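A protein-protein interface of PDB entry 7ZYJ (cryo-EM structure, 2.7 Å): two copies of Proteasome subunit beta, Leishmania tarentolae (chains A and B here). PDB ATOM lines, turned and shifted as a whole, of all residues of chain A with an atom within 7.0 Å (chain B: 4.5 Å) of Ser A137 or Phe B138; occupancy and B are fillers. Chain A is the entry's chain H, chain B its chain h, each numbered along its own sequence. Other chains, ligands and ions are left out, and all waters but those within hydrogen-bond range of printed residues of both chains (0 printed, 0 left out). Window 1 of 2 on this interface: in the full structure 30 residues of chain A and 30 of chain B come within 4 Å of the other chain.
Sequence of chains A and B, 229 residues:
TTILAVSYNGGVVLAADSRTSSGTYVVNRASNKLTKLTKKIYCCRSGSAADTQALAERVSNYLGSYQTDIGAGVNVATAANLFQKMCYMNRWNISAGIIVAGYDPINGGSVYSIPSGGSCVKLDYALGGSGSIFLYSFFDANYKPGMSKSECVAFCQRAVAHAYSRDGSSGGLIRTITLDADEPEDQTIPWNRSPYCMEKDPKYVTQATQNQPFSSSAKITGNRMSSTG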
ATOM      1  N   LEU A 127       2.361  28.911  15.214  1.00  0.00           N
ATOM      2  CA  LEU A 127       1.617  29.830  16.063  1.00  0.00           C
ATOM      3  C   LEU A 127       2.166  29.765  17.481  1.00  0.00           C
ATOM      4  O   LEU A 127       2.690  28.735  17.913  1.00  0.00           O
ATOM      5  CB  LEU A 127       0.121  29.495  16.073  1.00  0.00           C
ATOM      6  CG  LEU A 127      -0.524  29.140  14.733  1.00  0.00           C
ATOM      7  CD1 LEU A 127      -1.933  28.611  14.941  1.00  0.00           C
ATOM      8  CD2 LEU A 127      -0.536  30.340  13.804  1.00  0.00           C
ATOM      9  N   SER A 132      -2.598  32.240  20.421  1.00  0.00           N
ATOM     10  CA  SER A 132      -2.487  31.233  19.373  1.00  0.00           C
ATOM     11  C   SER A 132      -3.582  30.181  19.473  1.00  0.00           C
ATOM     12  O   SER A 132      -3.967  29.595  18.454  1.00  0.00           O
ATOM     13  CB  SER A 132      -1.117  30.560  19.431  1.00  0.00           C
ATOM     14  OG  SER A 132      -0.953  29.844  20.642  1.00  0.00           O
ATOM     15  N   ILE A 133      -4.095  29.937  20.681  1.00  0.00           N
ATOM     16  CA  ILE A 133      -5.106  28.904  20.880  1.00  0.00           C
ATOM     17  C   ILE A 133      -6.369  29.221  20.092  1.00  0.00           C
ATOM     18  O   ILE A 133      -7.128  28.316  19.726  1.00  0.00           O
ATOM     19  CB  ILE A 133      -5.396  28.737  22.387  1.00  0.00           C
ATOM     20  CG1 ILE A 133      -6.091  27.403  22.661  1.00  0.00           C
ATOM     21  CG2 ILE A 133      -6.222  29.902  22.918  1.00  0.00           C
ATOM     22  CD1 ILE A 133      -5.195  26.207  22.452  1.00  0.00           C
ATOM     23  N   PHE A 134      -6.614  30.501  19.810  1.00  0.00           N
ATOM     24  CA  PHE A 134      -7.782  30.908  19.042  1.00  0.00           C
ATOM     25  C   PHE A 134      -7.591  30.745  17.543  1.00  0.00           C
ATOM     26  O   PHE A 134      -8.578  30.810  16.804  1.00  0.00           O
ATOM     27  CB  PHE A 134      -8.121  32.365  19.349  1.00  0.00           C
ATOM     28  CG  PHE A 134      -8.386  32.627  20.798  1.00  0.00           C
ATOM     29  CD1 PHE A 134      -9.535  32.154  21.400  1.00  0.00           C
ATOM     30  CD2 PHE A 134      -7.478  33.340  21.561  1.00  0.00           C
ATOM     31  CE1 PHE A 134      -9.776  32.390  22.733  1.00  0.00           C
ATOM     32  CE2 PHE A 134      -7.716  33.579  22.897  1.00  0.00           C
ATOM     33  CZ  PHE A 134      -8.866  33.103  23.483  1.00  0.00           C
ATOM     34  N   LEU A 135      -6.362  30.533  17.076  1.00  0.00           N
ATOM     35  CA  LEU A 135      -6.082  30.576  15.649  1.00  0.00           C
ATOM     36  C   LEU A 135      -6.033  29.209  14.988  1.00  0.00           C
ATOM     37  O   LEU A 135      -6.110  29.138  13.757  1.00  0.00           O
ATOM     38  CB  LEU A 135      -4.755  31.295  15.393  1.00  0.00           C
ATOM     39  CG  LEU A 135      -4.828  32.815  15.505  1.00  0.00           C
ATOM     40  CD1 LEU A 135      -3.560  33.453  14.975  1.00  0.00           C
ATOM     41  CD2 LEU A 135      -6.048  33.329  14.764  1.00  0.00           C
ATOM     42  N   TYR A 136      -5.919  28.129  15.763  1.00  0.00           N
ATOM     43  CA  TYR A 136      -5.725  26.811  15.169  1.00  0.00           C
ATOM     44  C   TYR A 136      -6.893  26.443  14.264  1.00  0.00           C
ATOM     45  O   TYR A 136      -6.710  26.158  13.074  1.00  0.00           O
ATOM     46  CB  TYR A 136      -5.532  25.773  16.274  1.00  0.00           C
ATOM     47  CG  TYR A 136      -4.123  25.753  16.813  1.00  0.00           C
ATOM     48  CD1 TYR A 136      -3.099  25.138  16.107  1.00  0.00           C
ATOM     49  CD2 TYR A 136      -3.810  26.374  18.014  1.00  0.00           C
ATOM     50  CE1 TYR A 136      -1.807  25.127  16.591  1.00  0.00           C
ATOM     51  CE2 TYR A 136      -2.521  26.369  18.505  1.00  0.00           C
ATOM     52  CZ  TYR A 136      -1.523  25.743  17.789  1.00  0.00           C
ATOM     53  OH  TYR A 136      -0.237  25.735  18.273  1.00  0.00           O
ATOM     54  N   SER A 137      -8.116  26.506  14.797  1.00  0.00           N
ATOM     55  CA  SER A 137      -9.289  26.261  13.970  1.00  0.00           C
ATOM     56  C   SER A 137      -9.464  27.331  12.904  1.00  0.00           C
ATOM     57  O   SER A 137     -10.121  27.077  11.890  1.00  0.00           O
ATOM     58  CB  SER A 137     -10.544  26.177  14.838  1.00  0.00           C
ATOM     59  OG  SER A 137     -10.870  27.442  15.384  1.00  0.00           O
ATOM     60  N   PHE A 138      -8.892  28.520  13.110  1.00  0.00           N
ATOM     61  CA  PHE A 138      -8.887  29.519  12.051  1.00  0.00           C
ATOM     62  C   PHE A 138      -7.990  29.092  10.898  1.00  0.00           C
ATOM     63  O   PHE A 138      -8.307  29.361   9.734  1.00  0.00           O
ATOM     64  CB  PHE A 138      -8.443  30.874  12.603  1.00  0.00           C
ATOM     65  CG  PHE A 138      -8.495  31.987  11.594  1.00  0.00           C
ATOM     66  CD1 PHE A 138      -9.664  32.699  11.392  1.00  0.00           C
ATOM     67  CD2 PHE A 138      -7.375  32.326  10.855  1.00  0.00           C
ATOM     68  CE1 PHE A 138      -9.716  33.724  10.468  1.00  0.00           C
ATOM     69  CE2 PHE A 138      -7.421  33.349   9.929  1.00  0.00           C
ATOM     70  CZ  PHE A 138      -8.594  34.049   9.737  1.00  0.00           C
ATOM     71  N   PHE A 139      -6.868  28.432  11.196  1.00  0.00           N
ATOM     72  CA  PHE A 139      -5.988  27.968  10.133  1.00  0.00           C
ATOM     73  C   PHE A 139      -6.516  26.702   9.474  1.00  0.00           C
ATOM     74  O   PHE A 139      -6.302  26.496   8.276  1.00  0.00           O
ATOM     75  CB  PHE A 139      -4.579  27.738  10.676  1.00  0.00           C
ATOM     76  CG  PHE A 139      -3.697  28.949  10.593  1.00  0.00           C
ATOM     77  CD1 PHE A 139      -3.918  30.037  11.419  1.00  0.00           C
ATOM     78  CD2 PHE A 139      -2.655  29.005   9.684  1.00  0.00           C
ATOM     79  CE1 PHE A 139      -3.113  31.155  11.344  1.00  0.00           C
ATOM     80  CE2 PHE A 139      -1.846  30.120   9.605  1.00  0.00           C
ATOM     81  CZ  PHE A 139      -2.075  31.197  10.437  1.00  0.00           C
ATOM     82  N   ASP A 140      -7.206  25.850  10.234  1.00  0.00           N
ATOM     83  CA  ASP A 140      -7.747  24.623   9.663  1.00  0.00           C
ATOM     84  C   ASP A 140      -8.851  24.908   8.653  1.00  0.00           C
ATOM     85  O   ASP A 140      -9.069  24.111   7.735  1.00  0.00           O
ATOM     86  CB  ASP A 140      -8.269  23.718  10.776  1.00  0.00           C
ATOM     87  CG  ASP A 140      -7.180  23.280  11.729  1.00  0.00           C
ATOM     88  OD1 ASP A 140      -5.999  23.286  11.327  1.00  0.00           O
ATOM     89  OD2 ASP A 140      -7.505  22.928  12.882  1.00  0.00           O
ATOM     90  N   ALA A 141      -9.550  26.031   8.801  1.00  0.00           N
ATOM     91  CA  ALA A 141     -10.691  26.356   7.954  1.00  0.00           C
ATOM     92  C   ALA A 141     -10.369  27.359   6.856  1.00  0.00           C
ATOM     93  O   ALA A 141     -10.858  27.212   5.732  1.00  0.00           O
ATOM     94  CB  ALA A 141     -11.843  26.898   8.807  1.00  0.00           C
ATOM     95  N   ASN A 142      -9.560  28.378   7.147  1.00  0.00           N
ATOM     96  CA  ASN A 142      -9.376  29.494   6.233  1.00  0.00           C
ATOM     97  C   ASN A 142      -7.999  29.560   5.588  1.00  0.00           C
ATOM     98  O   ASN A 142      -7.816  30.344   4.652  1.00  0.00           O
ATOM     99  CB  ASN A 142      -9.649  30.820   6.958  1.00  0.00           C
ATOM    100  CG  ASN A 142     -11.036  30.876   7.562  1.00  0.00           C
ATOM    101  OD1 ASN A 142     -11.213  30.662   8.760  1.00  0.00           O
ATOM    102  ND2 ASN A 142     -12.030  31.165   6.732  1.00  0.00           N
ATOM    103  N   TYR A 143      -7.034  28.770   6.047  1.00  0.00           N
ATOM    104  CA  TYR A 143      -5.672  28.840   5.537  1.00  0.00           C
ATOM    105  C   TYR A 143      -5.471  27.809   4.436  1.00  0.00           C
ATOM    106  O   TYR A 143      -5.732  26.618   4.635  1.00  0.00           O
ATOM    107  CB  TYR A 143      -4.653  28.614   6.655  1.00  0.00           C
ATOM    108  CG  TYR A 143      -3.241  28.418   6.156  1.00  0.00           C
ATOM    109  CD1 TYR A 143      -2.487  29.494   5.712  1.00  0.00           C
ATOM    110  CD2 TYR A 143      -2.661  27.157   6.129  1.00  0.00           C
ATOM    111  CE1 TYR A 143      -1.199  29.320   5.254  1.00  0.00           C
ATOM    112  CE2 TYR A 143      -1.373  26.975   5.671  1.00  0.00           C
ATOM    113  CZ  TYR A 143      -0.647  28.060   5.236  1.00  0.00           C
ATOM    114  OH  TYR A 143       0.639  27.884   4.780  1.00  0.00           O
ATOM    115  N   HIS A 162      -7.995  38.545  14.336  1.00  0.00           N
ATOM    116  CA  HIS A 162      -8.952  37.601  14.901  1.00  0.00           C
ATOM    117  C   HIS A 162      -8.464  37.037  16.225  1.00  0.00           C
ATOM    118  O   HIS A 162      -9.271  36.766  17.122  1.00  0.00           O
ATOM    119  CB  HIS A 162      -9.220  36.469  13.910  1.00  0.00           C
ATOM    120  CG  HIS A 162     -10.359  36.740  12.977  1.00  0.00           C
ATOM    121  ND1 HIS A 162     -11.675  36.538  13.330  1.00  0.00           N
ATOM    122  CD2 HIS A 162     -10.377  37.193  11.702  1.00  0.00           C
ATOM    123  CE1 HIS A 162     -12.455  36.859  12.314  1.00  0.00           C
ATOM    124  NE2 HIS A 162     -11.692  37.258  11.313  1.00  0.00           N
ATOM    125  N   PHE B 134     -11.798  26.857  20.875  1.00  0.00           N
ATOM    126  CA  PHE B 134     -11.319  26.804  19.502  1.00  0.00           C
ATOM    127  C   PHE B 134     -12.311  27.379  18.504  1.00  0.00           C
ATOM    128  O   PHE B 134     -11.931  27.625  17.356  1.00  0.00           O
ATOM    129  CB  PHE B 134     -11.003  25.359  19.119  1.00  0.00           C
ATOM    130  CG  PHE B 134      -9.988  24.712  20.006  1.00  0.00           C
ATOM    131  CD1 PHE B 134      -8.661  25.094  19.954  1.00  0.00           C
ATOM    132  CD2 PHE B 134     -10.362  23.726  20.901  1.00  0.00           C
ATOM    133  CE1 PHE B 134      -7.730  24.504  20.773  1.00  0.00           C
ATOM    134  CE2 PHE B 134      -9.431  23.131  21.724  1.00  0.00           C
ATOM    135  CZ  PHE B 134      -8.112  23.520  21.659  1.00  0.00           C
ATOM    136  N   LEU B 135     -13.561  27.602  18.906  1.00  0.00           N
ATOM    137  CA  LEU B 135     -14.606  27.953  17.956  1.00  0.00           C
ATOM    138  C   LEU B 135     -14.893  29.443  17.874  1.00  0.00           C
ATOM    139  O   LEU B 135     -15.524  29.877  16.904  1.00  0.00           O
ATOM    140  CB  LEU B 135     -15.903  27.217  18.303  1.00  0.00           C
ATOM    141  CG  LEU B 135     -15.922  25.745  17.904  1.00  0.00           C
ATOM    142  CD1 LEU B 135     -17.320  25.174  18.030  1.00  0.00           C
ATOM    143  CD2 LEU B 135     -15.394  25.587  16.489  1.00  0.00           C
ATOM    144  N   TYR B 136     -14.444  30.232  18.850  1.00  0.00           N
ATOM    145  CA  TYR B 136     -14.816  31.642  18.889  1.00  0.00           C
ATOM    146  C   TYR B 136     -14.341  32.366  17.636  1.00  0.00           C
ATOM    147  O   TYR B 136     -15.141  32.968  16.908  1.00  0.00           O
ATOM    148  CB  TYR B 136     -14.248  32.289  20.152  1.00  0.00           C
ATOM    149  CG  TYR B 136     -15.092  32.018  21.372  1.00  0.00           C
ATOM    150  CD1 TYR B 136     -16.272  32.714  21.593  1.00  0.00           C
ATOM    151  CD2 TYR B 136     -14.723  31.046  22.292  1.00  0.00           C
ATOM    152  CE1 TYR B 136     -17.052  32.461  22.702  1.00  0.00           C
ATOM    153  CE2 TYR B 136     -15.497  30.787  23.403  1.00  0.00           C
ATOM    154  CZ  TYR B 136     -16.660  31.498  23.604  1.00  0.00           C
ATOM    155  OH  TYR B 136     -17.435  31.242  24.710  1.00  0.00           O
ATOM    156  N   SER B 137     -13.045  32.265  17.332  1.00  0.00           N
ATOM    157  CA  SER B 137     -12.534  32.850  16.100  1.00  0.00           C
ATOM    158  C   SER B 137     -13.097  32.159  14.869  1.00  0.00           C
ATOM    159  O   SER B 137     -13.114  32.758  13.790  1.00  0.00           O
ATOM    160  CB  SER B 137     -11.007  32.794  16.079  1.00  0.00           C
ATOM    161  OG  SER B 137     -10.550  31.462  15.944  1.00  0.00           O
ATOM    162  N   PHE B 138     -13.560  30.914  15.006  1.00  0.00           N
ATOM    163  CA  PHE B 138     -14.260  30.272  13.902  1.00  0.00           C
ATOM    164  C   PHE B 138     -15.609  30.930  13.651  1.00  0.00           C
ATOM    165  O   PHE B 138     -16.036  31.044  12.497  1.00  0.00           O
ATOM    166  CB  PHE B 138     -14.437  28.779  14.183  1.00  0.00           C
ATOM    167  CG  PHE B 138     -15.071  28.019  13.053  1.00  0.00           C
ATOM    168  CD1 PHE B 138     -14.299  27.511  12.024  1.00  0.00           C
ATOM    169  CD2 PHE B 138     -16.439  27.807  13.023  1.00  0.00           C
ATOM    170  CE1 PHE B 138     -14.877  26.810  10.986  1.00  0.00           C
ATOM    171  CE2 PHE B 138     -17.023  27.107  11.985  1.00  0.00           C
ATOM    172  CZ  PHE B 138     -16.240  26.608  10.966  1.00  0.00           C
ATOM    173  N   PHE B 139     -16.293  31.365  14.710  1.00  0.00           N
ATOM    174  CA  PHE B 139     -17.574  32.036  14.528  1.00  0.00           C
ATOM    175  C   PHE B 139     -17.398  33.481  14.091  1.00  0.00           C
ATOM    176  O   PHE B 139     -18.236  34.008  13.352  1.00  0.00           O
ATOM    177  CB  PHE B 139     -18.395  31.963  15.814  1.00  0.00           C
ATOM    178  CG  PHE B 139     -19.277  30.752  15.899  1.00  0.00           C
ATOM    179  CD1 PHE B 139     -18.729  29.496  16.091  1.00  0.00           C
ATOM    180  CD2 PHE B 139     -20.651  30.867  15.776  1.00  0.00           C
ATOM    181  CE1 PHE B 139     -19.534  28.379  16.165  1.00  0.00           C
ATOM    182  CE2 PHE B 139     -21.461  29.751  15.849  1.00  0.00           C
ATOM    183  CZ  PHE B 139     -20.901  28.506  16.045  1.00  0.00           C
ATOM    184  N   ASP B 140     -16.323  34.135  14.532  1.00  0.00           N
ATOM    185  CA  ASP B 140     -16.091  35.521  14.143  1.00  0.00           C
ATOM    186  C   ASP B 140     -15.790  35.649  12.656  1.00  0.00           C
ATOM    187  O   ASP B 140     -16.057  36.696  12.058  1.00  0.00           O
ATOM    188  CB  ASP B 140     -14.944  36.107  14.966  1.00  0.00           C
ATOM    189  CG  ASP B 140     -15.250  36.142  16.447  1.00  0.00           C
ATOM    190  OD1 ASP B 140     -16.446  36.143  16.808  1.00  0.00           O
ATOM    191  OD2 ASP B 140     -14.297  36.171  17.251  1.00  0.00           O
ATOM    192  N   ALA B 141     -15.239  34.603  12.044  1.00  0.00           N
ATOM    193  CA  ALA B 141     -14.818  34.647  10.650  1.00  0.00           C
ATOM    194  C   ALA B 141     -15.799  33.982   9.695  1.00  0.00           C
ATOM    195  O   ALA B 141     -16.025  34.496   8.595  1.00  0.00           O
ATOM    196  CB  ALA B 141     -13.442  33.991  10.494  1.00  0.00           C
ATOM    197  N   ASN B 142     -16.392  32.852  10.082  1.00  0.00           N
ATOM    198  CA  ASN B 142     -17.165  32.040   9.155  1.00  0.00           C
ATOM    199  C   ASN B 142     -18.663  32.037   9.419  1.00  0.00           C
ATOM    200  O   ASN B 142     -19.416  31.544   8.573  1.00  0.00           O
ATOM    201  CB  ASN B 142     -16.654  30.592   9.174  1.00  0.00           C
ATOM    202  CG  ASN B 142     -15.181  30.491   8.839  1.00  0.00           C
ATOM    203  OD1 ASN B 142     -14.338  30.363   9.725  1.00  0.00           O
ATOM    204  ND2 ASN B 142     -14.863  30.550   7.553  1.00  0.00           N
ATOM    205  N   TYR B 143     -19.120  32.565  10.549  1.00  0.00           N
ATOM    206  CA  TYR B 143     -20.530  32.517  10.909  1.00  0.00           C
ATOM    207  C   TYR B 143     -21.227  33.799  10.480  1.00  0.00           C
ATOM    208  O   TYR B 143     -20.810  34.897  10.861  1.00  0.00           O
ATOM    209  CB  TYR B 143     -20.708  32.301  12.411  1.00  0.00           C
ATOM    210  CG  TYR B 143     -22.128  32.500  12.888  1.00  0.00           C
ATOM    211  CD1 TYR B 143     -23.096  31.531  12.664  1.00  0.00           C
ATOM    212  CD2 TYR B 143     -22.499  33.651  13.567  1.00  0.00           C
ATOM    213  CE1 TYR B 143     -24.392  31.707  13.096  1.00  0.00           C
ATOM    214  CE2 TYR B 143     -23.795  33.836  14.002  1.00  0.00           C
ATOM    215  CZ  TYR B 143     -24.737  32.860  13.765  1.00  0.00           C
ATOM    216  OH  TYR B 143     -26.029  33.038  14.199  1.00  0.00           O
ATOM    217  N   PHE B 155     -23.557  24.093   9.309  1.00  0.00           N
ATOM    218  CA  PHE B 155     -22.546  24.920   9.954  1.00  0.00           C
ATOM    219  C   PHE B 155     -22.248  24.432  11.365  1.00  0.00           C
ATOM    220  O   PHE B 155     -21.091  24.444  11.795  1.00  0.00           O
ATOM    221  CB  PHE B 155     -22.987  26.383   9.977  1.00  0.00           C
ATOM    222  CG  PHE B 155     -21.939  27.315  10.510  1.00  0.00           C
ATOM    223  CD1 PHE B 155     -20.971  27.839   9.671  1.00  0.00           C
ATOM    224  CD2 PHE B 155     -21.916  27.663  11.850  1.00  0.00           C
ATOM    225  CE1 PHE B 155     -20.001  28.690  10.157  1.00  0.00           C
ATOM    226  CE2 PHE B 155     -20.948  28.514  12.341  1.00  0.00           C
ATOM    227  CZ  PHE B 155     -19.990  29.028  11.494  1.00  0.00           C
ATOM    228  N   ARG B 158     -20.068  21.349  11.052  1.00  0.00           N
ATOM    229  CA  ARG B 158     -18.718  21.734  10.656  1.00  0.00           C
ATOM    230  C   ARG B 158     -17.958  22.360  11.820  1.00  0.00           C
ATOM    231  O   ARG B 158     -16.769  22.082  12.020  1.00  0.00           O
ATOM    232  CB  ARG B 158     -18.787  22.692   9.468  1.00  0.00           C
ATOM    233  CG  ARG B 158     -17.463  22.966   8.787  1.00  0.00           C
ATOM    234  CD  ARG B 158     -17.617  24.065   7.749  1.00  0.00           C
ATOM    235  NE  ARG B 158     -16.345  24.688   7.406  1.00  0.00           N
ATOM    236  CZ  ARG B 158     -16.194  25.978   7.138  1.00  0.00           C
ATOM    237  NH1 ARG B 158     -17.219  26.814   7.169  1.00  0.00           N
ATOM    238  NH2 ARG B 158     -14.985  26.440   6.834  1.00  0.00           N
ATOM    239  N   ALA B 159     -18.633  23.207  12.602  1.00  0.00           N
ATOM    240  CA  ALA B 159     -17.999  23.825  13.759  1.00  0.00           C
ATOM    241  C   ALA B 159     -17.618  22.787  14.806  1.00  0.00           C
ATOM    242  O   ALA B 159     -16.529  22.856  15.382  1.00  0.00           O
ATOM    243  CB  ALA B 159     -18.923  24.882  14.361  1.00  0.00           C
ATOM    244  N   HIS B 162     -14.538  20.931  13.530  1.00  0.00           N
ATOM    245  CA  HIS B 162     -13.346  21.753  13.695  1.00  0.00           C
ATOM    246  C   HIS B 162     -12.939  21.858  15.157  1.00  0.00           C
ATOM    247  O   HIS B 162     -11.745  21.929  15.467  1.00  0.00           O
ATOM    248  CB  HIS B 162     -13.583  23.145  13.111  1.00  0.00           C
ATOM    249  CG  HIS B 162     -13.210  23.267  11.668  1.00  0.00           C
ATOM    250  ND1 HIS B 162     -11.913  23.479  11.250  1.00  0.00           N
ATOM    251  CD2 HIS B 162     -13.962  23.209  10.545  1.00  0.00           C
ATOM    252  CE1 HIS B 162     -11.884  23.543   9.932  1.00  0.00           C
ATOM    253  NE2 HIS B 162     -13.114  23.384   9.479  1.00  0.00           N
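The backbone carbonyl oxygen (O) of Phe B134 lies close to the side-chain hydroxyl (OG) of Ser A137, at 2.2 Å. The backbone carbonyl oxygen of Phe A134 sits close to the side-chain hydroxyl of Ser B137. The side-chain amide nitrogen of Asn A142 sits close to the side-chain amide nitrogen of Asn B142 (3.0 Å).
The side-chain amide oxygen of Asn B142 sits close to the backbone carbonyl oxygen of Phe B138, 3.3 Å away. The backbone carbonyl oxygen (O) of Phe A138 lies close to the side-chain amide oxygen (OD1) of Asn A142, at 3.3 Å.
Phe B134 touches Ile A133 (CE1 to CD1, 3.5 Å). OG of Ser A137 touches CB of Phe B138, 3.99 Å away. Ser B137 touches Phe A138 (OG to CB, 3.99 Å). Ala B141 touches Phe A138. Asp A140 touches His B162. Ala A141 touches Phe B138 (CB to CE1, 3.7 Å). Ala A141 touches Arg B158 (CB to NH2, 3.7 Å). His B162 touches Ala A141. CE1 of His A162 touches C of Asp B140, at 3.6 Å. His A162 touches Ala B141.
Printed residues of chain B within 4 Å of Ser A137: Phe B134 (2.2 Å) and Phe B138 (3.99 Å). Of the printed residues of chain A, Phe B138 touches Ser A137 and Ala A141. Printed residues of chain B within 4 Å of Phe A134: Ser B137. Of the printed residues of chain B, His A162 touches Asp B140 (3.6 Å) and Ala B141 (3.5 Å). Printed residues of chain A within 4 Å of Asn B142: Asn A142. Of the printed residues of chain B, Ala A141 touches Phe B138, Arg B158 and His B162. Tyr B143 touches none of the printed residues of chain A. Tyr B136 touches none of the printed residues of chain A. The nearest printed residue of chain B that does not touch Ser A137 is His B162 (4.1 Å). The nearest printed residue of chain A that does not touch Phe B138 is Phe A134 (5.3 Å).
Of the 14 printed residues of chain A, 8 touch a printed residue of chain B. Among the printed residues, no Asp or Glu carboxylate lies within 4 Å of a Lys or Arg side-chain nitrogen of the other chain.
Phe A134 touches Ser B137, and with the chains exchanged Ser A137 touches Phe B134. Asp A140 touches His B162, and with the chains exchanged His A162 touches Asp B140. Ala A141 touches His B162, and with the chains exchanged His A162 touches Ala B141. Asn A142 touches its own counterpart, Asn B142. 11 positions are printed for both chains.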
